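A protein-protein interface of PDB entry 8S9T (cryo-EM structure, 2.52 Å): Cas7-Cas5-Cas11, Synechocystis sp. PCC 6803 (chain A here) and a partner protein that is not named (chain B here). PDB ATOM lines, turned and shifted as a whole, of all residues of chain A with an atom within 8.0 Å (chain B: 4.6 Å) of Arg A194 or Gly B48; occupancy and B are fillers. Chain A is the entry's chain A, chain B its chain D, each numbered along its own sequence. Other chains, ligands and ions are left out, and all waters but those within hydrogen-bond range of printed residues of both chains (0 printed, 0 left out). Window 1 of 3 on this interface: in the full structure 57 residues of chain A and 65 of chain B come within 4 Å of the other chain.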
ATOM      1  N   SER A  12      18.981  16.043  -1.404  1.00  0.00           N
ATOM      2  CA  SER A  12      17.851  16.177  -2.300  1.00  0.00           C
ATOM      3  C   SER A  12      17.586  14.819  -2.923  1.00  0.00           C
ATOM      4  O   SER A  12      18.383  13.893  -2.787  1.00  0.00           O
ATOM      5  CB  SER A  12      18.093  17.248  -3.371  1.00  0.00           C
ATOM      6  OG  SER A  12      19.037  16.835  -4.329  1.00  0.00           O
ATOM      7  N   ASP A  13      16.425  14.687  -3.557  1.00  0.00           N
ATOM      8  CA  ASP A  13      16.106  13.453  -4.258  1.00  0.00           C
ATOM      9  C   ASP A  13      17.137  13.203  -5.344  1.00  0.00           C
ATOM     10  O   ASP A  13      17.662  14.126  -5.962  1.00  0.00           O
ATOM     11  CB  ASP A  13      14.712  13.509  -4.883  1.00  0.00           C
ATOM     12  CG  ASP A  13      13.643  13.946  -3.906  1.00  0.00           C
ATOM     13  OD1 ASP A  13      13.528  13.355  -2.821  1.00  0.00           O
ATOM     14  OD2 ASP A  13      12.907  14.896  -4.236  1.00  0.00           O
ATOM     15  N   LYS A 125       9.168  11.553 -10.909  1.00  0.00           N
ATOM     16  CA  LYS A 125       9.255  12.970 -11.190  1.00  0.00           C
ATOM     17  C   LYS A 125       8.875  13.221 -12.641  1.00  0.00           C
ATOM     18  O   LYS A 125       9.457  12.592 -13.534  1.00  0.00           O
ATOM     19  CB  LYS A 125      10.656  13.483 -10.911  1.00  0.00           C
ATOM     20  CG  LYS A 125      10.758  14.967 -10.941  1.00  0.00           C
ATOM     21  CD  LYS A 125      12.056  15.462 -10.373  1.00  0.00           C
ATOM     22  CE  LYS A 125      12.113  16.959 -10.474  1.00  0.00           C
ATOM     23  NZ  LYS A 125      13.259  17.537  -9.744  1.00  0.00           N
ATOM     24  N   GLU A 145      10.835  10.270 -14.624  1.00  0.00           N
ATOM     25  CA  GLU A 145      12.080   9.765 -14.068  1.00  0.00           C
ATOM     26  C   GLU A 145      11.844   9.261 -12.651  1.00  0.00           C
ATOM     27  O   GLU A 145      11.212   9.944 -11.843  1.00  0.00           O
ATOM     28  CB  GLU A 145      13.149  10.857 -14.084  1.00  0.00           C
ATOM     29  CG  GLU A 145      14.444  10.534 -13.364  1.00  0.00           C
ATOM     30  CD  GLU A 145      15.531  11.578 -13.603  1.00  0.00           C
ATOM     31  OE1 GLU A 145      16.171  11.554 -14.676  1.00  0.00           O
ATOM     32  OE2 GLU A 145      15.734  12.436 -12.722  1.00  0.00           O
ATOM     33  N   ARG A 187      27.350  17.201  -5.341  1.00  0.00           N
ATOM     34  CA  ARG A 187      26.376  16.538  -6.195  1.00  0.00           C
ATOM     35  C   ARG A 187      26.930  15.247  -6.752  1.00  0.00           C
ATOM     36  O   ARG A 187      28.133  15.105  -6.948  1.00  0.00           O
ATOM     37  CB  ARG A 187      25.975  17.425  -7.375  1.00  0.00           C
ATOM     38  CG  ARG A 187      25.095  18.517  -6.992  1.00  0.00           C
ATOM     39  CD  ARG A 187      24.991  19.614  -7.995  1.00  0.00           C
ATOM     40  NE  ARG A 187      24.530  20.753  -7.228  1.00  0.00           N
ATOM     41  CZ  ARG A 187      25.327  21.509  -6.496  1.00  0.00           C
ATOM     42  NH1 ARG A 187      26.635  21.365  -6.595  1.00  0.00           N
ATOM     43  NH2 ARG A 187      24.830  22.500  -5.785  1.00  0.00           N
ATOM     44  N   GLY A 190      22.440  11.561 -11.714  1.00  0.00           N
ATOM     45  CA  GLY A 190      21.784  12.139 -12.867  1.00  0.00           C
ATOM     46  C   GLY A 190      21.014  13.398 -12.541  1.00  0.00           C
ATOM     47  O   GLY A 190      20.385  13.515 -11.494  1.00  0.00           O
ATOM     48  N   LYS A 191      21.063  14.340 -13.477  1.00  0.00           N
ATOM     49  CA  LYS A 191      20.486  15.677 -13.355  1.00  0.00           C
ATOM     50  C   LYS A 191      21.021  16.444 -12.142  1.00  0.00           C
ATOM     51  O   LYS A 191      20.271  17.118 -11.438  1.00  0.00           O
ATOM     52  CB  LYS A 191      18.958  15.607 -13.327  1.00  0.00           C
ATOM     53  CG  LYS A 191      18.311  14.967 -14.553  1.00  0.00           C
ATOM     54  CD  LYS A 191      18.656  15.639 -15.874  1.00  0.00           C
ATOM     55  CE  LYS A 191      18.133  17.072 -15.985  1.00  0.00           C
ATOM     56  NZ  LYS A 191      18.533  17.733 -17.282  1.00  0.00           N
ATOM     57  N   ARG A 192      22.333  16.342 -11.905  1.00  0.00           N
ATOM     58  CA  ARG A 192      23.025  17.174 -10.919  1.00  0.00           C
ATOM     59  C   ARG A 192      22.742  18.654 -11.093  1.00  0.00           C
ATOM     60  O   ARG A 192      22.545  19.372 -10.115  1.00  0.00           O
ATOM     61  CB  ARG A 192      24.534  16.936 -11.019  1.00  0.00           C
ATOM     62  CG  ARG A 192      24.871  15.563 -10.852  1.00  0.00           C
ATOM     63  CD  ARG A 192      26.284  15.247 -10.453  1.00  0.00           C
ATOM     64  NE  ARG A 192      27.086  14.854 -11.602  1.00  0.00           N
ATOM     65  CZ  ARG A 192      28.306  15.272 -11.862  1.00  0.00           C
ATOM     66  NH1 ARG A 192      28.815  16.309 -11.226  1.00  0.00           N
ATOM     67  NH2 ARG A 192      28.921  14.793 -12.919  1.00  0.00           N
ATOM     68  N   ARG A 193      22.816  19.143 -12.328  1.00  0.00           N
ATOM     69  CA  ARG A 193      22.665  20.562 -12.628  1.00  0.00           C
ATOM     70  C   ARG A 193      21.241  21.069 -12.495  1.00  0.00           C
ATOM     71  O   ARG A 193      21.031  22.274 -12.600  1.00  0.00           O
ATOM     72  CB  ARG A 193      23.208  20.860 -14.025  1.00  0.00           C
ATOM     73  CG  ARG A 193      24.711  20.719 -14.119  1.00  0.00           C
ATOM     74  CD  ARG A 193      25.173  19.311 -14.408  1.00  0.00           C
ATOM     75  NE  ARG A 193      26.585  19.177 -14.078  1.00  0.00           N
ATOM     76  CZ  ARG A 193      27.325  18.101 -14.301  1.00  0.00           C
ATOM     77  NH1 ARG A 193      26.784  17.013 -14.792  1.00  0.00           N
ATOM     78  NH2 ARG A 193      28.594  18.102 -13.961  1.00  0.00           N
ATOM     79  N   ARG A 194      20.268  20.197 -12.264  1.00  0.00           N
ATOM     80  CA  ARG A 194      18.875  20.582 -12.072  1.00  0.00           C
ATOM     81  C   ARG A 194      18.356  20.165 -10.707  1.00  0.00           C
ATOM     82  O   ARG A 194      17.156  19.982 -10.535  1.00  0.00           O
ATOM     83  CB  ARG A 194      17.991  20.002 -13.171  1.00  0.00           C
ATOM     84  CG  ARG A 194      18.395  20.371 -14.558  1.00  0.00           C
ATOM     85  CD  ARG A 194      18.262  21.857 -14.788  1.00  0.00           C
ATOM     86  NE  ARG A 194      18.897  22.246 -16.037  1.00  0.00           N
ATOM     87  CZ  ARG A 194      19.936  23.061 -16.140  1.00  0.00           C
ATOM     88  NH1 ARG A 194      20.534  23.531 -15.062  1.00  0.00           N
ATOM     89  NH2 ARG A 194      20.419  23.342 -17.330  1.00  0.00           N
ATOM     90  N   GLY A 195      19.251  19.976  -9.750  1.00  0.00           N
ATOM     91  CA  GLY A 195      18.911  19.834  -8.358  1.00  0.00           C
ATOM     92  C   GLY A 195      18.766  18.431  -7.828  1.00  0.00           C
ATOM     93  O   GLY A 195      18.550  18.277  -6.625  1.00  0.00           O
ATOM     94  N   ASN A 196      18.874  17.407  -8.664  1.00  0.00           N
ATOM     95  CA  ASN A 196      19.057  16.056  -8.158  1.00  0.00           C
ATOM     96  C   ASN A 196      20.400  15.898  -7.459  1.00  0.00           C
ATOM     97  O   ASN A 196      21.383  16.564  -7.789  1.00  0.00           O
ATOM     98  CB  ASN A 196      18.949  15.032  -9.277  1.00  0.00           C
ATOM     99  CG  ASN A 196      17.525  14.711  -9.642  1.00  0.00           C
ATOM    100  OD1 ASN A 196      16.586  15.270  -9.089  1.00  0.00           O
ATOM    101  ND2 ASN A 196      17.358  13.803 -10.584  1.00  0.00           N
ATOM    102  N   GLY A 197      20.433  15.003  -6.481  1.00  0.00           N
ATOM    103  CA  GLY A 197      21.682  14.426  -6.031  1.00  0.00           C
ATOM    104  C   GLY A 197      22.540  15.283  -5.143  1.00  0.00           C
ATOM    105  O   GLY A 197      23.716  14.979  -4.972  1.00  0.00           O
ATOM    106  N   VAL B  46       9.904  23.457  -5.178  1.00  0.00           N
ATOM    107  CA  VAL B  46      10.140  23.800  -6.576  1.00  0.00           C
ATOM    108  C   VAL B  46      11.208  22.855  -7.109  1.00  0.00           C
ATOM    109  O   VAL B  46      12.340  22.886  -6.614  1.00  0.00           O
ATOM    110  CB  VAL B  46      10.560  25.267  -6.729  1.00  0.00           C
ATOM    111  CG1 VAL B  46      10.803  25.609  -8.181  1.00  0.00           C
ATOM    112  CG2 VAL B  46       9.493  26.145  -6.162  1.00  0.00           C
ATOM    113  N   PRO B  47      10.892  21.993  -8.070  1.00  0.00           N
ATOM    114  CA  PRO B  47      11.941  21.249  -8.777  1.00  0.00           C
ATOM    115  C   PRO B  47      12.889  22.177  -9.517  1.00  0.00           C
ATOM    116  O   PRO B  47      12.471  23.142 -10.152  1.00  0.00           O
ATOM    117  CB  PRO B  47      11.154  20.369  -9.751  1.00  0.00           C
ATOM    118  CG  PRO B  47       9.780  20.374  -9.277  1.00  0.00           C
ATOM    119  CD  PRO B  47       9.548  21.625  -8.529  1.00  0.00           C
ATOM    120  N   GLY B  48      14.183  21.894  -9.406  1.00  0.00           N
ATOM    121  CA  GLY B  48      15.170  22.652 -10.151  1.00  0.00           C
ATOM    122  C   GLY B  48      15.017  22.565 -11.656  1.00  0.00           C
ATOM    123  O   GLY B  48      15.418  23.476 -12.371  1.00  0.00           O
ATOM    124  N   THR B  49      14.445  21.473 -12.162  1.00  0.00           N
ATOM    125  CA  THR B  49      14.100  21.411 -13.581  1.00  0.00           C
ATOM    126  C   THR B  49      13.050  22.449 -13.956  1.00  0.00           C
ATOM    127  O   THR B  49      13.090  23.013 -15.049  1.00  0.00           O
ATOM    128  CB  THR B  49      13.622  20.011 -13.959  1.00  0.00           C
ATOM    129  OG1 THR B  49      14.566  19.049 -13.499  1.00  0.00           O
ATOM    130  CG2 THR B  49      13.498  19.875 -15.454  1.00  0.00           C
ATOM    131  N   SER B  50      12.073  22.673 -13.088  1.00  0.00           N
ATOM    132  CA  SER B  50      11.027  23.639 -13.389  1.00  0.00           C
ATOM    133  C   SER B  50      11.518  25.073 -13.212  1.00  0.00           C
ATOM    134  O   SER B  50      11.138  25.956 -13.981  1.00  0.00           O
ATOM    135  CB  SER B  50       9.789  23.342 -12.543  1.00  0.00           C
ATOM    136  OG  SER B  50       9.980  23.695 -11.197  1.00  0.00           O
ATOM    137  N   LEU B  51      12.348  25.331 -12.205  1.00  0.00           N
ATOM    138  CA  LEU B  51      12.941  26.654 -12.061  1.00  0.00           C
ATOM    139  C   LEU B  51      13.946  26.952 -13.164  1.00  0.00           C
ATOM    140  O   LEU B  51      14.013  28.082 -13.651  1.00  0.00           O
ATOM    141  CB  LEU B  51      13.604  26.795 -10.695  1.00  0.00           C
ATOM    142  CG  LEU B  51      14.270  28.141 -10.405  1.00  0.00           C
ATOM    143  CD1 LEU B  51      13.283  29.286 -10.458  1.00  0.00           C
ATOM    144  CD2 LEU B  51      14.928  28.111  -9.059  1.00  0.00           C
ATOM    145  N   ALA B  52      14.760  25.970 -13.548  1.00  0.00           N
ATOM    146  CA  ALA B  52      15.698  26.181 -14.641  1.00  0.00           C
ATOM    147  C   ALA B  52      14.991  26.565 -15.927  1.00  0.00           C
ATOM    148  O   ALA B  52      15.399  27.507 -16.611  1.00  0.00           O
ATOM    149  CB  ALA B  52      16.544  24.937 -14.867  1.00  0.00           C
ATOM    150  N   TRP B  74      23.389  27.142 -20.358  1.00  0.00           N
ATOM    151  CA  TRP B  74      22.477  26.100 -19.927  1.00  0.00           C
ATOM    152  C   TRP B  74      22.856  24.726 -20.444  1.00  0.00           C
ATOM    153  O   TRP B  74      22.202  23.750 -20.086  1.00  0.00           O
ATOM    154  CB  TRP B  74      21.059  26.462 -20.351  1.00  0.00           C
ATOM    155  CG  TRP B  74      20.622  27.714 -19.723  1.00  0.00           C
ATOM    156  CD1 TRP B  74      20.636  28.945 -20.280  1.00  0.00           C
ATOM    157  CD2 TRP B  74      20.152  27.883 -18.388  1.00  0.00           C
ATOM    158  NE1 TRP B  74      20.186  29.875 -19.389  1.00  0.00           N
ATOM    159  CE2 TRP B  74      19.883  29.249 -18.214  1.00  0.00           C
ATOM    160  CE3 TRP B  74      19.918  27.011 -17.325  1.00  0.00           C
ATOM    161  CZ2 TRP B  74      19.395  29.761 -17.030  1.00  0.00           C
ATOM    162  CZ3 TRP B  74      19.436  27.520 -16.158  1.00  0.00           C
ATOM    163  CH2 TRP B  74      19.178  28.881 -16.013  1.00  0.00           C
ATOM    164  N   SER B  85      25.363  21.937 -18.279  1.00  0.00           N
ATOM    165  CA  SER B  85      25.062  23.285 -17.823  1.00  0.00           C
ATOM    166  C   SER B  85      26.109  23.848 -16.866  1.00  0.00           C
ATOM    167  O   SER B  85      26.621  23.151 -15.992  1.00  0.00           O
ATOM    168  CB  SER B  85      23.712  23.287 -17.128  1.00  0.00           C
ATOM    169  OG  SER B  85      23.322  24.591 -16.806  1.00  0.00           O
ATOM    170  N   VAL B  87      25.149  26.695 -15.183  1.00  0.00           N
ATOM    171  CA  VAL B  87      24.208  26.969 -14.106  1.00  0.00           C
ATOM    172  C   VAL B  87      23.768  25.656 -13.471  1.00  0.00           C
ATOM    173  O   VAL B  87      23.276  24.761 -14.159  1.00  0.00           O
ATOM    174  CB  VAL B  87      23.001  27.757 -14.636  1.00  0.00           C
ATOM    175  CG1 VAL B  87      22.164  28.307 -13.496  1.00  0.00           C
ATOM    176  CG2 VAL B  87      23.459  28.856 -15.561  1.00  0.00           C
ATOM    177  N   VAL B  89      20.884  24.556 -10.860  1.00  0.00           N
ATOM    178  CA  VAL B  89      19.666  24.996 -10.193  1.00  0.00           C
ATOM    179  C   VAL B  89      19.241  23.897  -9.236  1.00  0.00           C
ATOM    180  O   VAL B  89      18.824  22.820  -9.670  1.00  0.00           O
ATOM    181  CB  VAL B  89      18.551  25.323 -11.199  1.00  0.00           C
ATOM    182  CG1 VAL B  89      17.375  25.950 -10.503  1.00  0.00           C
ATOM    183  CG2 VAL B  89      19.067  26.254 -12.271  1.00  0.00           C
ATOM    184  N   ASP B  90      19.350  24.157  -7.940  1.00  0.00           N
ATOM    185  CA  ASP B  90      18.904  23.220  -6.920  1.00  0.00           C
ATOM    186  C   ASP B  90      17.386  23.228  -6.744  1.00  0.00           C
ATOM    187  O   ASP B  90      16.685  24.147  -7.156  1.00  0.00           O
ATOM    188  CB  ASP B  90      19.584  23.518  -5.591  1.00  0.00           C
ATOM    189  CG  ASP B  90      20.942  22.891  -5.487  1.00  0.00           C
ATOM    190  OD1 ASP B  90      21.222  21.951  -6.254  1.00  0.00           O
ATOM    191  OD2 ASP B  90      21.742  23.337  -4.643  1.00  0.00           O
ATOM    192  N   ASP B  91      16.886  22.133  -6.178  1.00  0.00           N
ATOM    193  CA  ASP B  91      15.519  22.038  -5.682  1.00  0.00           C
ATOM    194  C   ASP B  91      15.336  22.897  -4.434  1.00  0.00           C
ATOM    195  O   ASP B  91      16.233  22.986  -3.594  1.00  0.00           O
ATOM    196  CB  ASP B  91      15.186  20.589  -5.359  1.00  0.00           C
ATOM    197  CG  ASP B  91      15.177  19.699  -6.582  1.00  0.00           C
ATOM    198  OD1 ASP B  91      14.935  20.190  -7.696  1.00  0.00           O
ATOM    199  OD2 ASP B  91      15.405  18.482  -6.425  1.00  0.00           O
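O of Val B89 is in hydrogen-bond range of N of Gly A195 (2.9 Å).
O of Arg A194 sits close to O of Val B89 (3.4 Å).
The backbone carbonyl oxygen (O) of Gly A195 sits close to the side-chain carboxylate (OD2) of Asp B91 (3.2 Å).
The guanidinium group (NH2) of Arg A194 lies within hydrogen-bond range of the side-chain hydroxyl (OG) of Ser B85.
O of Arg A193 lies within hydrogen-bond range of N of Val B89, at 2.9 Å.
OD1 of Asp B91 is in salt-bridge range of NZ of Lys A125, at 3.7 Å.
The backbone carbonyl oxygen (O) of Arg A194 lies within hydrogen-bond range of the backbone NH (N) of Thr B49, 3.5 Å away.
NH2 of Arg A194 lies within hydrogen-bond range of O of Trp B74, 3.3 Å away.
NH2 of Arg A187 lies within salt-bridge range of OD2 of Asp B90 (3.4 Å).
The backbone carbonyl oxygen (O) of Val B87 lies within hydrogen-bond range of the guanidinium group (NH1) of Arg A194, at 3.1 Å.
The backbone carbonyl oxygen (O) of Gly A195 is in hydrogen-bond range of the side-chain hydroxyl (OG) of Ser A12 (2.8 Å).
N of Lys A125 is in hydrogen-bond range of O of Glu A145.
OG of Ser B85 sits at hydrogen-bond distance from O of Val B87 (2.7 Å).
O of Pro B47 sits at hydrogen-bond distance from OG of Ser B50 (2.8 Å).
The backbone NH (N) of Gly B48 sits at hydrogen-bond distance from the side-chain carboxylate (OD1) of Asp B91 (2.5 Å).
CB of Pro B47 touches NZ of Lys A125, 3.5 Å away.
Arg A193 touches Ser B85 (CG to O, 3.6 Å).
O of Arg A193 touches O of Val B87 (3.7 Å).
Arg A194 touches Gly B48 (O to CA, 3.3 Å).
Ala B52 touches Arg A194.
Arg A194 touches Asp B91 (O to OD1, 3.6 Å).
Gly A195 touches Asp B90 (CA to CA, 3.7 Å).
Asp A13 touches none of the printed residues of chain B.
Printed residues of chain B within 4 Å of Arg A193: Ser B85 (3.6 Å), Val B87 (3.7 Å) and Val B89 (2.9 Å).
Arg A194 touches eight residues of chain B.
Of the printed residues of chain B, Gly A195 touches Val B89, Asp B90 and Asp B91.
Asn A196 touches none of the printed residues of chain B.
Of the printed residues of chain A, Gly B48 touches Arg A194.
Of the printed residues of chain A, Ala B52 touches Arg A194 (3.5 Å).
Of the printed residues of chain A, Asp B90 touches Arg A187 (3.4 Å) and Gly A195 (3.7 Å).
The nearest printed residue of chain A that does not touch Pro B47 is Arg A194 (4.9 Å).
Among the printed residues, 17 pairs touch across the chains.
Among the printed residues, Asp or Glu carboxylates within 4 Å of a Lys or Arg side-chain nitrogen of the other chain: Lys A125 with Asp B91 (3.7 Å) and Arg A187 with Asp B90 (3.4 Å).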
